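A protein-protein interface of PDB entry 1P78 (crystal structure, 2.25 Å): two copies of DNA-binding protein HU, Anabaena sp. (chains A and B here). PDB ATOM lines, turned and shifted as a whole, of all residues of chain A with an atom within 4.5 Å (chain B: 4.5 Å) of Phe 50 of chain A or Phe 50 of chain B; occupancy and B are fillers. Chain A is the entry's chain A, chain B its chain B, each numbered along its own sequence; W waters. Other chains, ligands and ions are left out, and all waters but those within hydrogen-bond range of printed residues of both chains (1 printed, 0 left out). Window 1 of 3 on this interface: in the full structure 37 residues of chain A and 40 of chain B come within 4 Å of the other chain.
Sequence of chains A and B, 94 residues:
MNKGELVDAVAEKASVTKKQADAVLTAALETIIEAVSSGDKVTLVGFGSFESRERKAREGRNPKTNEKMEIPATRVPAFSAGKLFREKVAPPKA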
ATOM      1  N   ILE A  32      -2.621  -2.642  31.275  1.00  0.00           N
ATOM      2  CA  ILE A  32      -3.008  -4.029  31.512  1.00  0.00           C
ATOM      3  C   ILE A  32      -1.767  -4.939  31.445  1.00  0.00           C
ATOM      4  O   ILE A  32      -1.454  -5.639  32.420  1.00  0.00           O
ATOM      5  CB  ILE A  32      -4.132  -4.476  30.528  1.00  0.00           C
ATOM      6  CG1 ILE A  32      -5.472  -3.828  30.923  1.00  0.00           C
ATOM      7  CG2 ILE A  32      -4.276  -6.014  30.503  1.00  0.00           C
ATOM      8  CD1 ILE A  32      -6.577  -4.049  29.933  1.00  0.00           C
ATOM      9  N   VAL A  36       0.052  -7.140  34.533  1.00  0.00           N
ATOM     10  CA  VAL A  36       0.112  -8.593  34.416  1.00  0.00           C
ATOM     11  C   VAL A  36       1.548  -9.096  34.466  1.00  0.00           C
ATOM     12  O   VAL A  36       1.850 -10.010  35.228  1.00  0.00           O
ATOM     13  CB  VAL A  36      -0.623  -9.102  33.132  1.00  0.00           C
ATOM     14  CG1 VAL A  36      -0.431 -10.622  32.926  1.00  0.00           C
ATOM     15  CG2 VAL A  36      -2.109  -8.753  33.167  1.00  0.00           C
ATOM     16  N   ASP A  40       0.703  -8.637  38.652  1.00  0.00           N
ATOM     17  CA  ASP A  40      -0.612  -8.258  39.157  1.00  0.00           C
ATOM     18  C   ASP A  40      -1.741  -8.879  38.362  1.00  0.00           C
ATOM     19  O   ASP A  40      -1.618  -9.092  37.166  1.00  0.00           O
ATOM     20  CB  ASP A  40      -0.791  -6.739  39.197  1.00  0.00           C
ATOM     21  CG  ASP A  40      -1.754  -6.288  40.296  1.00  0.00           C
ATOM     22  OD1 ASP A  40      -2.140  -5.099  40.278  1.00  0.00           O
ATOM     23  OD2 ASP A  40      -2.171  -7.038  41.217  1.00  0.00           O
ATOM     24  N   LYS A  41      -2.845  -9.165  39.037  1.00  0.00           N
ATOM     25  CA  LYS A  41      -4.080  -9.565  38.368  1.00  0.00           C
ATOM     26  C   LYS A  41      -4.841  -8.302  37.954  1.00  0.00           C
ATOM     27  O   LYS A  41      -5.140  -7.460  38.804  1.00  0.00           O
ATOM     28  CB  LYS A  41      -4.935 -10.399  39.326  1.00  0.00           C
ATOM     29  CG  LYS A  41      -5.901 -11.336  38.615  1.00  0.00           C
ATOM     30  CD  LYS A  41      -6.668 -12.230  39.604  1.00  0.00           C
ATOM     31  CE  LYS A  41      -7.934 -12.786  38.954  1.00  0.00           C
ATOM     32  NZ  LYS A  41      -8.436 -14.043  39.600  1.00  0.00           N
ATOM     33  N   VAL A  42      -5.129  -8.137  36.664  1.00  0.00           N
ATOM     34  CA  VAL A  42      -6.053  -7.077  36.257  1.00  0.00           C
ATOM     35  C   VAL A  42      -7.482  -7.609  36.297  1.00  0.00           C
ATOM     36  O   VAL A  42      -7.816  -8.581  35.627  1.00  0.00           O
ATOM     37  CB  VAL A  42      -5.765  -6.500  34.871  1.00  0.00           C
ATOM     38  CG1 VAL A  42      -6.858  -5.491  34.486  1.00  0.00           C
ATOM     39  CG2 VAL A  42      -4.401  -5.844  34.820  1.00  0.00           C
ATOM     40  N   LEU A  44     -11.588  -6.759  35.762  1.00  0.00           N
ATOM     41  CA  LEU A  44     -12.563  -5.873  35.160  1.00  0.00           C
ATOM     42  C   LEU A  44     -13.924  -6.532  35.291  1.00  0.00           C
ATOM     43  O   LEU A  44     -14.292  -7.386  34.492  1.00  0.00           O
ATOM     44  CB  LEU A  44     -12.194  -5.612  33.706  1.00  0.00           C
ATOM     45  CG  LEU A  44     -10.758  -5.157  33.446  1.00  0.00           C
ATOM     46  CD1 LEU A  44     -10.440  -5.255  31.979  1.00  0.00           C
ATOM     47  CD2 LEU A  44     -10.556  -3.720  33.952  1.00  0.00           C
ATOM     48  N   PHE A  47     -16.451  -8.157  32.516  1.00  0.00           N
ATOM     49  CA  PHE A  47     -15.752  -8.445  31.274  1.00  0.00           C
ATOM     50  C   PHE A  47     -14.845  -9.679  31.493  1.00  0.00           C
ATOM     51  O   PHE A  47     -14.875 -10.646  30.708  1.00  0.00           O
ATOM     52  CB  PHE A  47     -14.952  -7.210  30.837  1.00  0.00           C
ATOM     53  CG  PHE A  47     -14.158  -7.400  29.580  1.00  0.00           C
ATOM     54  CD1 PHE A  47     -14.767  -7.301  28.346  1.00  0.00           C
ATOM     55  CD2 PHE A  47     -12.791  -7.663  29.636  1.00  0.00           C
ATOM     56  CE1 PHE A  47     -14.044  -7.470  27.165  1.00  0.00           C
ATOM     57  CE2 PHE A  47     -12.044  -7.830  28.469  1.00  0.00           C
ATOM     58  CZ  PHE A  47     -12.678  -7.741  27.222  1.00  0.00           C
ATOM     59  N   SER A  49     -10.946 -11.123  33.914  1.00  0.00           N
ATOM     60  CA  SER A  49      -9.645 -10.791  34.470  1.00  0.00           C
ATOM     61  C   SER A  49      -8.460 -11.238  33.577  1.00  0.00           C
ATOM     62  O   SER A  49      -8.601 -12.131  32.702  1.00  0.00           O
ATOM     63  CB  SER A  49      -9.509 -11.376  35.884  1.00  0.00           C
ATOM     64  OG  SER A  49      -9.724 -12.775  35.856  1.00  0.00           O
ATOM     65  N   PHE A  50      -7.316 -10.595  33.807  1.00  0.00           N
ATOM     66  CA  PHE A  50      -6.055 -10.984  33.204  1.00  0.00           C
ATOM     67  C   PHE A  50      -5.065 -11.317  34.316  1.00  0.00           C
ATOM     68  O   PHE A  50      -5.046 -10.672  35.368  1.00  0.00           O
ATOM     69  CB  PHE A  50      -5.483  -9.872  32.333  1.00  0.00           C
ATOM     70  CG  PHE A  50      -6.325  -9.526  31.144  1.00  0.00           C
ATOM     71  CD1 PHE A  50      -7.414  -8.675  31.265  1.00  0.00           C
ATOM     72  CD2 PHE A  50      -6.008 -10.036  29.892  1.00  0.00           C
ATOM     73  CE1 PHE A  50      -8.193  -8.356  30.148  1.00  0.00           C
ATOM     74  CE2 PHE A  50      -6.775  -9.713  28.769  1.00  0.00           C
ATOM     75  CZ  PHE A  50      -7.870  -8.881  28.898  1.00  0.00           C
ATOM     76  N   GLU A  51      -4.275 -12.361  34.099  1.00  0.00           N
ATOM     77  CA  GLU A  51      -3.207 -12.711  35.040  1.00  0.00           C
ATOM     78  C   GLU A  51      -2.105 -13.417  34.320  1.00  0.00           C
ATOM     79  O   GLU A  51      -2.275 -13.869  33.203  1.00  0.00           O
ATOM     80  CB  GLU A  51      -3.690 -13.564  36.213  1.00  0.00           C
ATOM     81  CG  GLU A  51      -4.356 -14.883  35.842  1.00  0.00           C
ATOM     82  CD  GLU A  51      -4.755 -15.660  37.082  1.00  0.00           C
ATOM     83  OE1 GLU A  51      -5.468 -15.092  37.953  1.00  0.00           O
ATOM     84  OE2 GLU A  51      -4.323 -16.825  37.230  1.00  0.00           O
ATOM     85  N   ALA A  78      -2.734 -14.839  30.892  1.00  0.00           N
ATOM     86  CA  ALA A  78      -3.973 -15.607  30.879  1.00  0.00           C
ATOM     87  C   ALA A  78      -5.180 -14.706  31.067  1.00  0.00           C
ATOM     88  O   ALA A  78      -5.119 -13.773  31.852  1.00  0.00           O
ATOM     89  CB  ALA A  78      -3.932 -16.612  31.974  1.00  0.00           C
ATOM     90  N   PHE A  79      -6.275 -15.005  30.365  1.00  0.00           N
ATOM     91  CA  PHE A  79      -7.551 -14.299  30.516  1.00  0.00           C
ATOM     92  C   PHE A  79      -8.681 -15.211  31.055  1.00  0.00           C
ATOM     93  O   PHE A  79      -8.737 -16.369  30.726  1.00  0.00           O
ATOM     94  CB  PHE A  79      -7.945 -13.692  29.167  1.00  0.00           C
ATOM     95  CG  PHE A  79      -9.284 -12.971  29.168  1.00  0.00           C
ATOM     96  CD1 PHE A  79      -9.465 -11.800  29.911  1.00  0.00           C
ATOM     97  CD2 PHE A  79     -10.365 -13.487  28.445  1.00  0.00           C
ATOM     98  CE1 PHE A  79     -10.682 -11.134  29.929  1.00  0.00           C
ATOM     99  CE2 PHE A  79     -11.608 -12.832  28.424  1.00  0.00           C
ATOM    100  CZ  PHE A  79     -11.765 -11.643  29.177  1.00  0.00           C
ATOM    101  N   PHE A  85     -19.724 -11.338  30.008  1.00  0.00           N
ATOM    102  CA  PHE A  85     -19.106 -11.693  28.729  1.00  0.00           C
ATOM    103  C   PHE A  85     -19.536 -13.116  28.284  1.00  0.00           C
ATOM    104  O   PHE A  85     -20.020 -13.303  27.165  1.00  0.00           O
ATOM    105  CB  PHE A  85     -17.580 -11.548  28.852  1.00  0.00           C
ATOM    106  CG  PHE A  85     -16.843 -11.458  27.527  1.00  0.00           C
ATOM    107  CD1 PHE A  85     -17.470 -11.780  26.324  1.00  0.00           C
ATOM    108  CD2 PHE A  85     -15.492 -11.079  27.504  1.00  0.00           C
ATOM    109  CE1 PHE A  85     -16.771 -11.726  25.106  1.00  0.00           C
ATOM    110  CE2 PHE A  85     -14.790 -11.015  26.302  1.00  0.00           C
ATOM    111  CZ  PHE A  85     -15.434 -11.337  25.097  1.00  0.00           C
ATOM    112  N   ILE B  32     -16.289  -4.744  22.639  1.00  0.00           N
ATOM    113  CA  ILE B  32     -15.542  -5.984  22.467  1.00  0.00           C
ATOM    114  C   ILE B  32     -16.497  -7.159  22.656  1.00  0.00           C
ATOM    115  O   ILE B  32     -16.584  -8.027  21.799  1.00  0.00           O
ATOM    116  CB  ILE B  32     -14.371  -6.100  23.468  1.00  0.00           C
ATOM    117  CG1 ILE B  32     -13.256  -5.099  23.124  1.00  0.00           C
ATOM    118  CG2 ILE B  32     -13.829  -7.522  23.452  1.00  0.00           C
ATOM    119  CD1 ILE B  32     -12.174  -4.886  24.241  1.00  0.00           C
ATOM    120  N   VAL B  36     -17.594  -9.839  19.704  1.00  0.00           N
ATOM    121  CA  VAL B  36     -17.216 -11.236  19.875  1.00  0.00           C
ATOM    122  C   VAL B  36     -18.466 -12.108  19.841  1.00  0.00           C
ATOM    123  O   VAL B  36     -18.481 -13.102  19.121  1.00  0.00           O
ATOM    124  CB  VAL B  36     -16.380 -11.444  21.176  1.00  0.00           C
ATOM    125  CG1 VAL B  36     -16.381 -12.907  21.633  1.00  0.00           C
ATOM    126  CG2 VAL B  36     -14.950 -10.897  20.988  1.00  0.00           C
ATOM    127  N   ASP B  40     -17.858 -11.598  15.648  1.00  0.00           N
ATOM    128  CA  ASP B  40     -16.780 -10.725  15.189  1.00  0.00           C
ATOM    129  C   ASP B  40     -15.523 -10.886  16.025  1.00  0.00           C
ATOM    130  O   ASP B  40     -15.544 -10.592  17.216  1.00  0.00           O
ATOM    131  CB  ASP B  40     -17.230  -9.259  15.278  1.00  0.00           C
ATOM    132  CG  ASP B  40     -16.487  -8.337  14.304  1.00  0.00           C
ATOM    133  OD1 ASP B  40     -16.930  -7.161  14.137  1.00  0.00           O
ATOM    134  OD2 ASP B  40     -15.464  -8.696  13.665  1.00  0.00           O
ATOM    135  N   LYS B  41     -14.429 -11.325  15.404  1.00  0.00           N
ATOM    136  CA  LYS B  41     -13.126 -11.388  16.072  1.00  0.00           C
ATOM    137  C   LYS B  41     -12.460 -10.014  16.327  1.00  0.00           C
ATOM    138  O   LYS B  41     -12.116  -9.308  15.382  1.00  0.00           O
ATOM    139  CB  LYS B  41     -12.166 -12.253  15.265  1.00  0.00           C
ATOM    140  CG  LYS B  41     -10.889 -12.509  16.021  1.00  0.00           C
ATOM    141  CD  LYS B  41      -9.928 -13.365  15.193  1.00  0.00           C
ATOM    142  CE  LYS B  41      -8.519 -13.348  15.803  1.00  0.00           C
ATOM    143  NZ  LYS B  41      -7.402 -13.558  14.798  1.00  0.00           N
ATOM    144  N   VAL B  42     -12.260  -9.646  17.589  1.00  0.00           N
ATOM    145  CA  VAL B  42     -11.628  -8.362  17.879  1.00  0.00           C
ATOM    146  C   VAL B  42     -10.111  -8.503  17.991  1.00  0.00           C
ATOM    147  O   VAL B  42      -9.607  -9.244  18.844  1.00  0.00           O
ATOM    148  CB  VAL B  42     -12.203  -7.694  19.131  1.00  0.00           C
ATOM    149  CG1 VAL B  42     -11.578  -6.324  19.312  1.00  0.00           C
ATOM    150  CG2 VAL B  42     -13.718  -7.566  19.016  1.00  0.00           C
ATOM    151  N   PHE B  47      -1.470  -6.200  21.525  1.00  0.00           N
ATOM    152  CA  PHE B  47      -2.123  -6.668  22.740  1.00  0.00           C
ATOM    153  C   PHE B  47      -2.606  -8.110  22.583  1.00  0.00           C
ATOM    154  O   PHE B  47      -2.143  -9.021  23.276  1.00  0.00           O
ATOM    155  CB  PHE B  47      -3.279  -5.745  23.106  1.00  0.00           C
ATOM    156  CG  PHE B  47      -3.923  -6.085  24.400  1.00  0.00           C
ATOM    157  CD1 PHE B  47      -3.307  -5.759  25.598  1.00  0.00           C
ATOM    158  CD2 PHE B  47      -5.149  -6.753  24.428  1.00  0.00           C
ATOM    159  CE1 PHE B  47      -3.905  -6.061  26.815  1.00  0.00           C
ATOM    160  CE2 PHE B  47      -5.761  -7.083  25.643  1.00  0.00           C
ATOM    161  CZ  PHE B  47      -5.143  -6.737  26.841  1.00  0.00           C
ATOM    162  N   GLY B  48      -3.536  -8.313  21.657  1.00  0.00           N
ATOM    163  CA  GLY B  48      -4.079  -9.630  21.421  1.00  0.00           C
ATOM    164  C   GLY B  48      -5.461  -9.586  20.832  1.00  0.00           C
ATOM    165  O   GLY B  48      -6.008  -8.519  20.523  1.00  0.00           O
ATOM    166  N   SER B  49      -6.036 -10.762  20.668  1.00  0.00           N
ATOM    167  CA  SER B  49      -7.309 -10.844  20.035  1.00  0.00           C
ATOM    168  C   SER B  49      -8.331 -11.585  20.875  1.00  0.00           C
ATOM    169  O   SER B  49      -7.990 -12.466  21.636  1.00  0.00           O
ATOM    170  CB  SER B  49      -7.145 -11.502  18.675  1.00  0.00           C
ATOM    171  OG  SER B  49      -6.567 -12.767  18.860  1.00  0.00           O
ATOM    172  N   PHE B  50      -9.593 -11.201  20.705  1.00  0.00           N
ATOM    173  CA  PHE B  50     -10.728 -11.860  21.331  1.00  0.00           C
ATOM    174  C   PHE B  50     -11.612 -12.498  20.246  1.00  0.00           C
ATOM    175  O   PHE B  50     -11.830 -11.930  19.165  1.00  0.00           O
ATOM    176  CB  PHE B  50     -11.544 -10.860  22.143  1.00  0.00           C
ATOM    177  CG  PHE B  50     -10.795 -10.219  23.283  1.00  0.00           C
ATOM    178  CD1 PHE B  50     -10.020  -9.079  23.081  1.00  0.00           C
ATOM    179  CD2 PHE B  50     -10.901 -10.736  24.568  1.00  0.00           C
ATOM    180  CE1 PHE B  50      -9.350  -8.470  24.142  1.00  0.00           C
ATOM    181  CE2 PHE B  50     -10.218 -10.154  25.626  1.00  0.00           C
ATOM    182  CZ  PHE B  50      -9.439  -9.012  25.422  1.00  0.00           C
ATOM    183  N   GLU B  51     -12.110 -13.693  20.532  1.00  0.00           N
ATOM    184  CA  GLU B  51     -13.013 -14.389  19.635  1.00  0.00           C
ATOM    185  C   GLU B  51     -13.827 -15.342  20.463  1.00  0.00           C
ATOM    186  O   GLU B  51     -13.498 -15.639  21.594  1.00  0.00           O
ATOM    187  CB  GLU B  51     -12.246 -15.172  18.553  1.00  0.00           C
ATOM    188  CG  GLU B  51     -11.453 -16.374  19.093  1.00  0.00           C
ATOM    189  CD  GLU B  51     -10.606 -17.113  18.039  1.00  0.00           C
ATOM    190  OE1 GLU B  51     -10.464 -16.644  16.873  1.00  0.00           O
ATOM    191  OE2 GLU B  51     -10.069 -18.197  18.382  1.00  0.00           O
ATOM    192  N   ALA B  78     -12.712 -16.349  23.951  1.00  0.00           N
ATOM    193  CA  ALA B  78     -11.296 -16.742  24.036  1.00  0.00           C
ATOM    194  C   ALA B  78     -10.407 -15.551  23.762  1.00  0.00           C
ATOM    195  O   ALA B  78     -10.759 -14.673  22.965  1.00  0.00           O
ATOM    196  CB  ALA B  78     -10.960 -17.892  23.062  1.00  0.00           C
ATOM    197  N   PHE B  79      -9.280 -15.514  24.444  1.00  0.00           N
ATOM    198  CA  PHE B  79      -8.322 -14.443  24.288  1.00  0.00           C
ATOM    199  C   PHE B  79      -7.032 -15.068  23.808  1.00  0.00           C
ATOM    200  O   PHE B  79      -6.609 -16.143  24.255  1.00  0.00           O
ATOM    201  CB  PHE B  79      -8.095 -13.711  25.608  1.00  0.00           C
ATOM    202  CG  PHE B  79      -7.002 -12.654  25.567  1.00  0.00           C
ATOM    203  CD1 PHE B  79      -7.097 -11.555  24.723  1.00  0.00           C
ATOM    204  CD2 PHE B  79      -5.900 -12.733  26.436  1.00  0.00           C
ATOM    205  CE1 PHE B  79      -6.104 -10.554  24.722  1.00  0.00           C
ATOM    206  CE2 PHE B  79      -4.904 -11.747  26.451  1.00  0.00           C
ATOM    207  CZ  PHE B  79      -5.000 -10.663  25.595  1.00  0.00           C
ATOM    208  N   PHE B  85       2.754  -8.904  24.314  1.00  0.00           N
ATOM    209  CA  PHE B  85       2.249  -9.277  25.635  1.00  0.00           C
ATOM    210  C   PHE B  85       3.028 -10.485  26.218  1.00  0.00           C
ATOM    211  O   PHE B  85       3.556 -10.423  27.320  1.00  0.00           O
ATOM    212  CB  PHE B  85       0.731  -9.536  25.547  1.00  0.00           C
ATOM    213  CG  PHE B  85       0.012  -9.466  26.870  1.00  0.00           C
ATOM    214  CD1 PHE B  85       0.717  -9.525  28.085  1.00  0.00           C
ATOM    215  CD2 PHE B  85      -1.373  -9.364  26.907  1.00  0.00           C
ATOM    216  CE1 PHE B  85       0.051  -9.468  29.300  1.00  0.00           C
ATOM    217  CE2 PHE B  85      -2.046  -9.311  28.128  1.00  0.00           C
ATOM    218  CZ  PHE B  85      -1.328  -9.366  29.319  1.00  0.00           C
HETATM  219  O   HOH W   1      -5.794 -16.710  27.600  1.00  0.00           O
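Hydrophobic or aromatic side chains of chain A within 4 Å of the printed part of chain B: Ile 32, Val 36, Phe 47, Phe 50, Phe 79 and Phe 85.
Hydrophobic or aromatic side chains of chain B within 4 Å of the printed part of chain A: Ile 32, Val 36, Phe 47, Phe 50, Phe 79 and Phe 85.
Among the printed residues, no Asp or Glu carboxylate lies within 4 Å of a Lys or Arg side-chain nitrogen of the other chain.
Phe 47 of chain B touches Ile 32 of chain A (CE1 to CG2, 3.7 Å).
Val 36 of chain A touches Phe 85 of chain B.
CE1 of Phe 47 of chain A touches CG2 of Ile 32 of chain B, 3.7 Å away.
Phe 47 of chain A touches Phe 50 of chain B.
Phe 47 of chain B touches Phe 50 of chain A.
CZ of Phe 50 of chain B touches CZ of Phe 50 of chain A, at 3.8 Å.
Phe 50 of chain A touches Phe 79 of chain B (CE2 to CE2, 3.6 Å).
Phe 79 of chain B touches Phe 79 of chain A (CD2 to CB, 3.5 Å).
Val 36 of chain B touches Phe 85 of chain A.
Water W1 bridges the backbone NH of Phe 79 of chain A (3.3 Å) and the backbone carbonyl oxygen of Phe 79 of chain B (3.5 Å).
Of the printed residues of chain B, Phe 47 of chain A touches Ile 32 (3.7 Å) and Phe 50 (3.8 Å).
Of chain B, only Phe 47, Phe 50 and Phe 79 come within 4 Å of Phe 50 of chain A.
Glu 51 of chain A touches none of the printed residues of chain B.
Printed residues of chain A within 4 Å of Ile 32 of chain B: Phe 47 (3.7 Å).
Printed residues of chain A within 4 Å of Val 36 of chain B: Phe 85 (3.7 Å).
Phe 50 of chain B touches just these residues of chain A: Phe 47 and Phe 50.
The nearest residue of chain B that does not touch Phe 50 of chain A is Phe 85 of chain B (4.4 Å).
The nearest residue of chain A that does not touch Phe 50 of chain B is Phe 79 of chain A (4.1 Å).
The nearest printed residue of chain B that does not touch Phe 47 of chain A is Phe 47 of chain B (6.9 Å).
Ile 32 of chain A touches Phe 47 of chain B, and with the chains exchanged Phe 47 of chain A touches Ile 32 of chain B.
Val 36 of chain A touches Phe 85 of chain B, and with the chains exchanged Phe 85 of chain A touches Val 36 of chain B.
Phe 47 of chain A touches Phe 50 of chain B, and with the chains exchanged Phe 50 of chain A touches Phe 47 of chain B.
Phe 50 of chain A touches its own counterpart, Phe 50 of chain B.
Positions printed for both chains: 32, 36, 40, 41, 42, 47, 49, 50, 51, 78, 79 and 85.
Of the 9 pairs that touch across the chains among the printed residues, 8 have their exchanged pair printed and touching as well.
The backbone NH (N) of Phe 50 of chain B is in hydrogen-bond range of the backbone carbonyl oxygen (O) of Val 42 of chain B (2.7 Å).
The backbone carbonyl oxygen (O) of Val 42 of chain A lies within hydrogen-bond range of the backbone NH (N) of Phe 50 of chain A (2.8 Å).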
